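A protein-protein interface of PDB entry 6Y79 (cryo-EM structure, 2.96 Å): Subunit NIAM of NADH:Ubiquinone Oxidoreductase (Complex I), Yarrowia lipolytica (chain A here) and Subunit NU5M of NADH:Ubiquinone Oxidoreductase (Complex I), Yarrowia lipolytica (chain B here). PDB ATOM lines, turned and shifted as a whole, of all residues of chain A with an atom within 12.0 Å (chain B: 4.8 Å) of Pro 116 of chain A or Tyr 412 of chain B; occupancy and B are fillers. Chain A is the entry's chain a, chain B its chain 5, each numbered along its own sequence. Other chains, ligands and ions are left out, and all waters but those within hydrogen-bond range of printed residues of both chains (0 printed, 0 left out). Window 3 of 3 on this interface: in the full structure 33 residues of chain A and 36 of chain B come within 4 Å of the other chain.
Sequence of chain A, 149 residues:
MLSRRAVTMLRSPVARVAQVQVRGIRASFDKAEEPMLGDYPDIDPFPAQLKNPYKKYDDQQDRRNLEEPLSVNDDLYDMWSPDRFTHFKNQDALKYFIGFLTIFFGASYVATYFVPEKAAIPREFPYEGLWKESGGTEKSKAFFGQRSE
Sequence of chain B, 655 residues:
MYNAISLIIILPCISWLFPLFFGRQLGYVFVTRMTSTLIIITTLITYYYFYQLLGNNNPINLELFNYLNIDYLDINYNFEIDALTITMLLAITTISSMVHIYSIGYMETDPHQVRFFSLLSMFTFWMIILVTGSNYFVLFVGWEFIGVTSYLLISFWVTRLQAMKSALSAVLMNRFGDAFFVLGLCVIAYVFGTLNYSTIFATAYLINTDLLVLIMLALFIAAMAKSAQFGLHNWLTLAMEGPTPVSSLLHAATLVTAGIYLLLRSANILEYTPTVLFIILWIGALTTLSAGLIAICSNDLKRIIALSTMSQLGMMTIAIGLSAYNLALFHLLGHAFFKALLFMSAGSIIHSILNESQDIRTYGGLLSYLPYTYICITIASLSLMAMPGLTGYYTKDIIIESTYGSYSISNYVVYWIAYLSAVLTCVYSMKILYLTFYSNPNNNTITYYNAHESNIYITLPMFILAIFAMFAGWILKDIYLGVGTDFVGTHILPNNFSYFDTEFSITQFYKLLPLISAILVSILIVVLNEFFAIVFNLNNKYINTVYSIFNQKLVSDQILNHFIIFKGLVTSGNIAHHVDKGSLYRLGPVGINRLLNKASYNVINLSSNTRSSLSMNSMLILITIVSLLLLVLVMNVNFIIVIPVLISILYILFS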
ATOM      1  N   PHE A 104     -38.287 -17.138   5.067  1.00  0.00           N
ATOM      2  CA  PHE A 104     -37.522 -18.381   5.041  1.00  0.00           C
ATOM      3  C   PHE A 104     -36.420 -18.349   3.993  1.00  0.00           C
ATOM      4  O   PHE A 104     -35.281 -18.709   4.288  1.00  0.00           O
ATOM      5  CB  PHE A 104     -38.442 -19.575   4.793  1.00  0.00           C
ATOM      6  CG  PHE A 104     -37.738 -20.894   4.818  1.00  0.00           C
ATOM      7  CD1 PHE A 104     -37.383 -21.474   6.021  1.00  0.00           C
ATOM      8  CD2 PHE A 104     -37.428 -21.554   3.641  1.00  0.00           C
ATOM      9  CE1 PHE A 104     -36.736 -22.687   6.046  1.00  0.00           C
ATOM     10  CE2 PHE A 104     -36.782 -22.764   3.665  1.00  0.00           C
ATOM     11  CZ  PHE A 104     -36.438 -23.330   4.868  1.00  0.00           C
ATOM     12  N   ALA A 107     -33.587 -15.800   5.030  1.00  0.00           N
ATOM     13  CA  ALA A 107     -32.729 -16.379   6.062  1.00  0.00           C
ATOM     14  C   ALA A 107     -31.915 -17.550   5.518  1.00  0.00           C
ATOM     15  O   ALA A 107     -30.757 -17.743   5.919  1.00  0.00           O
ATOM     16  CB  ALA A 107     -33.564 -16.807   7.267  1.00  0.00           C
ATOM     17  N   SER A 108     -32.487 -18.303   4.566  1.00  0.00           N
ATOM     18  CA  SER A 108     -31.780 -19.409   3.937  1.00  0.00           C
ATOM     19  C   SER A 108     -30.574 -18.895   3.171  1.00  0.00           C
ATOM     20  O   SER A 108     -29.479 -19.451   3.269  1.00  0.00           O
ATOM     21  CB  SER A 108     -32.719 -20.159   2.990  1.00  0.00           C
ATOM     22  OG  SER A 108     -33.991 -20.420   3.579  1.00  0.00           O
ATOM     23  N   TYR A 109     -30.753 -17.812   2.428  1.00  0.00           N
ATOM     24  CA  TYR A 109     -29.695 -17.343   1.547  1.00  0.00           C
ATOM     25  C   TYR A 109     -28.635 -16.543   2.300  1.00  0.00           C
ATOM     26  O   TYR A 109     -27.455 -16.591   1.938  1.00  0.00           O
ATOM     27  CB  TYR A 109     -30.317 -16.538   0.413  1.00  0.00           C
ATOM     28  CG  TYR A 109     -29.340 -16.047  -0.602  1.00  0.00           C
ATOM     29  CD1 TYR A 109     -28.774 -16.912  -1.528  1.00  0.00           C
ATOM     30  CD2 TYR A 109     -29.010 -14.707  -0.658  1.00  0.00           C
ATOM     31  CE1 TYR A 109     -27.889 -16.447  -2.475  1.00  0.00           C
ATOM     32  CE2 TYR A 109     -28.133 -14.234  -1.593  1.00  0.00           C
ATOM     33  CZ  TYR A 109     -27.574 -15.106  -2.498  1.00  0.00           C
ATOM     34  OH  TYR A 109     -26.697 -14.628  -3.435  1.00  0.00           O
ATOM     35  N   VAL A 110     -29.022 -15.800   3.344  1.00  0.00           N
ATOM     36  CA  VAL A 110     -27.996 -15.118   4.128  1.00  0.00           C
ATOM     37  C   VAL A 110     -27.244 -16.115   4.999  1.00  0.00           C
ATOM     38  O   VAL A 110     -26.083 -15.882   5.348  1.00  0.00           O
ATOM     39  CB  VAL A 110     -28.576 -13.953   4.966  1.00  0.00           C
ATOM     40  CG1 VAL A 110     -29.308 -12.948   4.077  1.00  0.00           C
ATOM     41  CG2 VAL A 110     -29.443 -14.430   6.129  1.00  0.00           C
ATOM     42  N   ALA A 111     -27.864 -17.248   5.344  1.00  0.00           N
ATOM     43  CA  ALA A 111     -27.177 -18.205   6.203  1.00  0.00           C
ATOM     44  C   ALA A 111     -26.162 -19.062   5.458  1.00  0.00           C
ATOM     45  O   ALA A 111     -25.429 -19.816   6.106  1.00  0.00           O
ATOM     46  CB  ALA A 111     -28.195 -19.094   6.911  1.00  0.00           C
ATOM     47  N   THR A 112     -26.106 -18.972   4.128  1.00  0.00           N
ATOM     48  CA  THR A 112     -25.064 -19.640   3.359  1.00  0.00           C
ATOM     49  C   THR A 112     -23.728 -18.909   3.486  1.00  0.00           C
ATOM     50  O   THR A 112     -22.669 -19.530   3.347  1.00  0.00           O
ATOM     51  CB  THR A 112     -25.547 -19.757   1.899  1.00  0.00           C
ATOM     52  OG1 THR A 112     -26.795 -20.459   1.884  1.00  0.00           O
ATOM     53  CG2 THR A 112     -24.571 -20.517   0.995  1.00  0.00           C
ATOM     54  N   TYR A 113     -23.747 -17.618   3.816  1.00  0.00           N
ATOM     55  CA  TYR A 113     -22.502 -16.870   3.942  1.00  0.00           C
ATOM     56  C   TYR A 113     -21.780 -17.130   5.256  1.00  0.00           C
ATOM     57  O   TYR A 113     -20.555 -16.998   5.306  1.00  0.00           O
ATOM     58  CB  TYR A 113     -22.776 -15.374   3.783  1.00  0.00           C
ATOM     59  CG  TYR A 113     -23.209 -15.018   2.387  1.00  0.00           C
ATOM     60  CD1 TYR A 113     -22.282 -14.919   1.357  1.00  0.00           C
ATOM     61  CD2 TYR A 113     -24.548 -14.799   2.090  1.00  0.00           C
ATOM     62  CE1 TYR A 113     -22.674 -14.602   0.071  1.00  0.00           C
ATOM     63  CE2 TYR A 113     -24.950 -14.482   0.809  1.00  0.00           C
ATOM     64  CZ  TYR A 113     -24.010 -14.386  -0.196  1.00  0.00           C
ATOM     65  OH  TYR A 113     -24.402 -14.069  -1.473  1.00  0.00           O
ATOM     66  N   PHE A 114     -22.496 -17.510   6.310  1.00  0.00           N
ATOM     67  CA  PHE A 114     -21.897 -17.690   7.629  1.00  0.00           C
ATOM     68  C   PHE A 114     -21.593 -19.154   7.922  1.00  0.00           C
ATOM     69  O   PHE A 114     -21.696 -19.590   9.071  1.00  0.00           O
ATOM     70  CB  PHE A 114     -22.808 -17.114   8.711  1.00  0.00           C
ATOM     71  CG  PHE A 114     -22.981 -15.615   8.649  1.00  0.00           C
ATOM     72  CD1 PHE A 114     -22.061 -14.807   7.995  1.00  0.00           C
ATOM     73  CD2 PHE A 114     -24.073 -15.014   9.263  1.00  0.00           C
ATOM     74  CE1 PHE A 114     -22.234 -13.435   7.944  1.00  0.00           C
ATOM     75  CE2 PHE A 114     -24.248 -13.642   9.219  1.00  0.00           C
ATOM     76  CZ  PHE A 114     -23.328 -12.854   8.559  1.00  0.00           C
ATOM     77  N   VAL A 115     -21.224 -19.946   6.919  1.00  0.00           N
ATOM     78  CA  VAL A 115     -20.999 -21.370   7.156  1.00  0.00           C
ATOM     79  C   VAL A 115     -19.534 -21.638   7.480  1.00  0.00           C
ATOM     80  O   VAL A 115     -18.648 -20.870   7.074  1.00  0.00           O
ATOM     81  CB  VAL A 115     -21.477 -22.234   5.973  1.00  0.00           C
ATOM     82  CG1 VAL A 115     -22.914 -21.919   5.638  1.00  0.00           C
ATOM     83  CG2 VAL A 115     -20.591 -22.062   4.745  1.00  0.00           C
ATOM     84  N   PRO A 116     -19.250 -22.672   8.265  1.00  0.00           N
ATOM     85  CA  PRO A 116     -17.886 -23.174   8.389  1.00  0.00           C
ATOM     86  C   PRO A 116     -17.615 -24.232   7.336  1.00  0.00           C
ATOM     87  O   PRO A 116     -18.523 -24.842   6.767  1.00  0.00           O
ATOM     88  CB  PRO A 116     -17.876 -23.790   9.791  1.00  0.00           C
ATOM     89  CG  PRO A 116     -19.250 -24.312   9.934  1.00  0.00           C
ATOM     90  CD  PRO A 116     -20.138 -23.299   9.253  1.00  0.00           C
ATOM     91  N   GLU A 117     -16.331 -24.400   7.044  1.00  0.00           N
ATOM     92  CA  GLU A 117     -15.908 -25.363   6.038  1.00  0.00           C
ATOM     93  C   GLU A 117     -15.249 -26.585   6.679  1.00  0.00           C
ATOM     94  O   GLU A 117     -15.135 -26.706   7.902  1.00  0.00           O
ATOM     95  CB  GLU A 117     -14.957 -24.738   5.008  1.00  0.00           C
ATOM     96  CG  GLU A 117     -15.480 -23.490   4.273  1.00  0.00           C
ATOM     97  CD  GLU A 117     -15.330 -22.218   5.082  1.00  0.00           C
ATOM     98  OE1 GLU A 117     -16.093 -21.255   4.856  1.00  0.00           O
ATOM     99  OE2 GLU A 117     -14.425 -22.196   5.935  1.00  0.00           O
ATOM    100  N   LYS A 118     -14.770 -27.477   5.815  1.00  0.00           N
ATOM    101  CA  LYS A 118     -14.774 -28.911   6.070  1.00  0.00           C
ATOM    102  C   LYS A 118     -13.607 -29.284   6.940  1.00  0.00           C
ATOM    103  O   LYS A 118     -12.677 -28.509   7.166  1.00  0.00           O
ATOM    104  CB  LYS A 118     -14.706 -29.757   4.786  1.00  0.00           C
ATOM    105  CG  LYS A 118     -16.040 -30.062   4.103  1.00  0.00           C
ATOM    106  CD  LYS A 118     -16.561 -28.763   3.518  1.00  0.00           C
ATOM    107  CE  LYS A 118     -17.956 -28.785   3.041  1.00  0.00           C
ATOM    108  NZ  LYS A 118     -18.468 -27.417   3.364  1.00  0.00           N
ATOM    109  N   ALA A 119     -13.656 -30.517   7.400  1.00  0.00           N
ATOM    110  CA  ALA A 119     -12.562 -31.069   8.149  1.00  0.00           C
ATOM    111  C   ALA A 119     -11.892 -32.236   7.441  1.00  0.00           C
ATOM    112  O   ALA A 119     -11.000 -32.861   8.021  1.00  0.00           O
ATOM    113  CB  ALA A 119     -13.054 -31.477   9.533  1.00  0.00           C
ATOM    114  N   ALA A 120     -12.294 -32.548   6.210  1.00  0.00           N
ATOM    115  CA  ALA A 120     -11.656 -33.562   5.382  1.00  0.00           C
ATOM    116  C   ALA A 120     -11.609 -33.080   3.938  1.00  0.00           C
ATOM    117  O   ALA A 120     -12.318 -32.142   3.563  1.00  0.00           O
ATOM    118  CB  ALA A 120     -12.402 -34.902   5.464  1.00  0.00           C
ATOM    119  N   THR B 403     -26.937 -34.480   6.640  1.00  0.00           N
ATOM    120  CA  THR B 403     -26.938 -33.099   6.163  1.00  0.00           C
ATOM    121  C   THR B 403     -25.607 -32.408   6.453  1.00  0.00           C
ATOM    122  O   THR B 403     -25.138 -31.597   5.647  1.00  0.00           O
ATOM    123  CB  THR B 403     -28.084 -32.314   6.788  1.00  0.00           C
ATOM    124  OG1 THR B 403     -27.995 -32.415   8.205  1.00  0.00           O
ATOM    125  CG2 THR B 403     -29.415 -32.866   6.352  1.00  0.00           C
ATOM    126  N   TYR B 404     -24.980 -32.714   7.594  1.00  0.00           N
ATOM    127  CA  TYR B 404     -23.699 -32.087   7.915  1.00  0.00           C
ATOM    128  C   TYR B 404     -22.540 -32.736   7.176  1.00  0.00           C
ATOM    129  O   TYR B 404     -21.667 -32.034   6.655  1.00  0.00           O
ATOM    130  CB  TYR B 404     -23.428 -32.136   9.420  1.00  0.00           C
ATOM    131  CG  TYR B 404     -22.088 -31.534   9.806  1.00  0.00           C
ATOM    132  CD1 TYR B 404     -21.917 -30.160   9.843  1.00  0.00           C
ATOM    133  CD2 TYR B 404     -20.996 -32.340  10.129  1.00  0.00           C
ATOM    134  CE1 TYR B 404     -20.702 -29.600  10.179  1.00  0.00           C
ATOM    135  CE2 TYR B 404     -19.774 -31.788  10.468  1.00  0.00           C
ATOM    136  CZ  TYR B 404     -19.636 -30.418  10.494  1.00  0.00           C
ATOM    137  OH  TYR B 404     -18.428 -29.854  10.835  1.00  0.00           O
ATOM    138  N   ILE B 409     -21.351 -27.490   0.369  1.00  0.00           N
ATOM    139  CA  ILE B 409     -21.098 -26.637   1.522  1.00  0.00           C
ATOM    140  C   ILE B 409     -22.415 -26.187   2.166  1.00  0.00           C
ATOM    141  O   ILE B 409     -22.604 -26.322   3.387  1.00  0.00           O
ATOM    142  CB  ILE B 409     -20.145 -25.479   1.130  1.00  0.00           C
ATOM    143  CG1 ILE B 409     -20.786 -24.340   0.304  1.00  0.00           C
ATOM    144  CG2 ILE B 409     -18.978 -26.054   0.333  1.00  0.00           C
ATOM    145  CD1 ILE B 409     -19.916 -23.141   0.228  1.00  0.00           C
ATOM    146  N   SER B 410     -23.393 -25.769   1.354  1.00  0.00           N
ATOM    147  CA  SER B 410     -24.595 -25.126   1.864  1.00  0.00           C
ATOM    148  C   SER B 410     -25.617 -26.120   2.381  1.00  0.00           C
ATOM    149  O   SER B 410     -26.635 -25.697   2.940  1.00  0.00           O
ATOM    150  CB  SER B 410     -25.211 -24.230   0.777  1.00  0.00           C
ATOM    151  OG  SER B 410     -25.637 -24.970  -0.350  1.00  0.00           O
ATOM    152  N   ASN B 411     -25.343 -27.423   2.250  1.00  0.00           N
ATOM    153  CA  ASN B 411     -26.048 -28.449   3.005  1.00  0.00           C
ATOM    154  C   ASN B 411     -25.952 -28.234   4.501  1.00  0.00           C
ATOM    155  O   ASN B 411     -26.861 -28.667   5.223  1.00  0.00           O
ATOM    156  CB  ASN B 411     -25.508 -29.846   2.712  1.00  0.00           C
ATOM    157  CG  ASN B 411     -25.815 -30.314   1.326  1.00  0.00           C
ATOM    158  OD1 ASN B 411     -24.951 -30.816   0.616  1.00  0.00           O
ATOM    159  ND2 ASN B 411     -27.054 -30.151   0.926  1.00  0.00           N
ATOM    160  N   TYR B 412     -24.879 -27.578   4.966  1.00  0.00           N
ATOM    161  CA  TYR B 412     -24.776 -27.192   6.364  1.00  0.00           C
ATOM    162  C   TYR B 412     -25.996 -26.405   6.828  1.00  0.00           C
ATOM    163  O   TYR B 412     -26.487 -26.647   7.938  1.00  0.00           O
ATOM    164  CB  TYR B 412     -23.510 -26.372   6.582  1.00  0.00           C
ATOM    165  CG  TYR B 412     -23.310 -25.990   8.014  1.00  0.00           C
ATOM    166  CD1 TYR B 412     -22.832 -26.915   8.923  1.00  0.00           C
ATOM    167  CD2 TYR B 412     -23.613 -24.713   8.463  1.00  0.00           C
ATOM    168  CE1 TYR B 412     -22.652 -26.583  10.238  1.00  0.00           C
ATOM    169  CE2 TYR B 412     -23.445 -24.374   9.772  1.00  0.00           C
ATOM    170  CZ  TYR B 412     -22.956 -25.312  10.657  1.00  0.00           C
ATOM    171  OH  TYR B 412     -22.776 -24.976  11.976  1.00  0.00           O
ATOM    172  N   VAL B 413     -26.544 -25.543   5.959  1.00  0.00           N
ATOM    173  CA  VAL B 413     -27.718 -24.756   6.321  1.00  0.00           C
ATOM    174  C   VAL B 413     -28.913 -25.660   6.574  1.00  0.00           C
ATOM    175  O   VAL B 413     -29.620 -25.497   7.580  1.00  0.00           O
ATOM    176  CB  VAL B 413     -28.027 -23.709   5.239  1.00  0.00           C
ATOM    177  CG1 VAL B 413     -29.187 -22.834   5.672  1.00  0.00           C
ATOM    178  CG2 VAL B 413     -26.808 -22.873   4.962  1.00  0.00           C
ATOM    179  N   VAL B 414     -29.106 -26.688   5.735  1.00  0.00           N
ATOM    180  CA  VAL B 414     -30.252 -27.554   5.973  1.00  0.00           C
ATOM    181  C   VAL B 414     -30.023 -28.452   7.171  1.00  0.00           C
ATOM    182  O   VAL B 414     -31.016 -28.941   7.729  1.00  0.00           O
ATOM    183  CB  VAL B 414     -30.682 -28.406   4.753  1.00  0.00           C
ATOM    184  CG1 VAL B 414     -30.722 -27.579   3.499  1.00  0.00           C
ATOM    185  CG2 VAL B 414     -29.838 -29.634   4.568  1.00  0.00           C
ATOM    186  N   TYR B 415     -28.754 -28.603   7.612  1.00  0.00           N
ATOM    187  CA  TYR B 415     -28.467 -29.221   8.905  1.00  0.00           C
ATOM    188  C   TYR B 415     -29.262 -28.556  10.000  1.00  0.00           C
ATOM    189  O   TYR B 415     -29.902 -29.232  10.804  1.00  0.00           O
ATOM    190  CB  TYR B 415     -26.981 -29.154   9.278  1.00  0.00           C
ATOM    191  CG  TYR B 415     -26.736 -29.756  10.662  1.00  0.00           C
ATOM    192  CD1 TYR B 415     -26.725 -31.121  10.827  1.00  0.00           C
ATOM    193  CD2 TYR B 415     -26.550 -28.968  11.799  1.00  0.00           C
ATOM    194  CE1 TYR B 415     -26.535 -31.705  12.058  1.00  0.00           C
ATOM    195  CE2 TYR B 415     -26.369 -29.547  13.044  1.00  0.00           C
ATOM    196  CZ  TYR B 415     -26.357 -30.920  13.160  1.00  0.00           C
ATOM    197  OH  TYR B 415     -26.165 -31.524  14.380  1.00  0.00           O
ATOM    198  N   TRP B 416     -29.254 -27.223  10.026  1.00  0.00           N
ATOM    199  CA  TRP B 416     -29.986 -26.537  11.073  1.00  0.00           C
ATOM    200  C   TRP B 416     -31.481 -26.639  10.850  1.00  0.00           C
ATOM    201  O   TRP B 416     -32.226 -26.813  11.821  1.00  0.00           O
ATOM    202  CB  TRP B 416     -29.534 -25.084  11.164  1.00  0.00           C
ATOM    203  CG  TRP B 416     -28.149 -24.990  11.679  1.00  0.00           C
ATOM    204  CD1 TRP B 416     -27.014 -24.875  10.945  1.00  0.00           C
ATOM    205  CD2 TRP B 416     -27.739 -25.046  13.047  1.00  0.00           C
ATOM    206  NE1 TRP B 416     -25.921 -24.839  11.770  1.00  0.00           N
ATOM    207  CE2 TRP B 416     -26.339 -24.942  13.066  1.00  0.00           C
ATOM    208  CE3 TRP B 416     -28.423 -25.165  14.260  1.00  0.00           C
ATOM    209  CZ2 TRP B 416     -25.606 -24.952  14.247  1.00  0.00           C
ATOM    210  CZ3 TRP B 416     -27.696 -25.177  15.430  1.00  0.00           C
ATOM    211  CH2 TRP B 416     -26.300 -25.070  15.416  1.00  0.00           C
ATOM    212  N   TYR B 510     -21.993 -31.973  17.455  1.00  0.00           N
ATOM    213  CA  TYR B 510     -23.043 -32.040  16.444  1.00  0.00           C
ATOM    214  C   TYR B 510     -23.803 -33.362  16.491  1.00  0.00           C
ATOM    215  O   TYR B 510     -24.958 -33.418  16.060  1.00  0.00           O
ATOM    216  CB  TYR B 510     -22.452 -31.825  15.053  1.00  0.00           C
ATOM    217  CG  TYR B 510     -22.008 -30.412  14.762  1.00  0.00           C
ATOM    218  CD1 TYR B 510     -22.582 -29.331  15.415  1.00  0.00           C
ATOM    219  CD2 TYR B 510     -21.001 -30.161  13.838  1.00  0.00           C
ATOM    220  CE1 TYR B 510     -22.170 -28.036  15.151  1.00  0.00           C
ATOM    221  CE2 TYR B 510     -20.582 -28.872  13.572  1.00  0.00           C
ATOM    222  CZ  TYR B 510     -21.172 -27.817  14.230  1.00  0.00           C
ATOM    223  OH  TYR B 510     -20.761 -26.533  13.970  1.00  0.00           O
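OG1 of Thr 112 of chain A is in hydrogen-bond range of O of Ser 108 of chain A. The indole nitrogen (NE1) of Trp 416 of chain B sits at hydrogen-bond distance from the side-chain hydroxyl (OH) of Tyr 412 of chain B, 3.2 Å away. OH of Tyr 412 of chain B lies within hydrogen-bond range of OH of Tyr 510 of chain B.
Hydrophobic or aromatic side chains of chain B within 4 Å of the printed part of chain A: Ile 409, Tyr 412 and Val 413. Printed residues of chain A that touch a printed residue of chain B: Ala 111, Thr 112, Pro 116 and Lys 118. Along chain A the printed residues that touch a printed residue of chain B span positions 111 to 118. Among the printed residues, 5 pairs touch across the chains.
Ala 111 of chain A touches Val 413 of chain B (O to CG2, 3.5 Å). Ser 410 of chain B touches Thr 112 of chain A (CB to CG2, 3.8 Å). Thr 112 of chain A touches Val 413 of chain B. Pro 116 of chain A touches Tyr 412 of chain B. Lys 118 of chain A touches Ile 409 of chain B.
Printed residues of chain B within 4 Å of Ala 111 of chain A: Val 413 (3.5 Å). Of the printed residues of chain B, Thr 112 of chain A touches Ser 410 (3.8 Å) and Val 413 (3.9 Å). No residue of chain A comes within 4 Å of Thr 403 of chain B. No residue of chain A comes within 4 Å of Tyr 404 of chain B. Printed residues of chain A within 4 Å of Ile 409 of chain B: Lys 118 (3.3 Å). Tyr 412 of chain B touches one residue of chain A. Val 413 of chain B touches two residues of chain A. No residue of chain A comes within 4 Å of Val 414 of chain B. No residue of chain A comes within 4 Å of Trp 416 of chain B. Tyr 510 of chain B touches none of the printed residues of chain A. The nearest printed residue of chain B that does not touch Pro 116 of chain A is Tyr 510 of chain B (4.8 Å).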
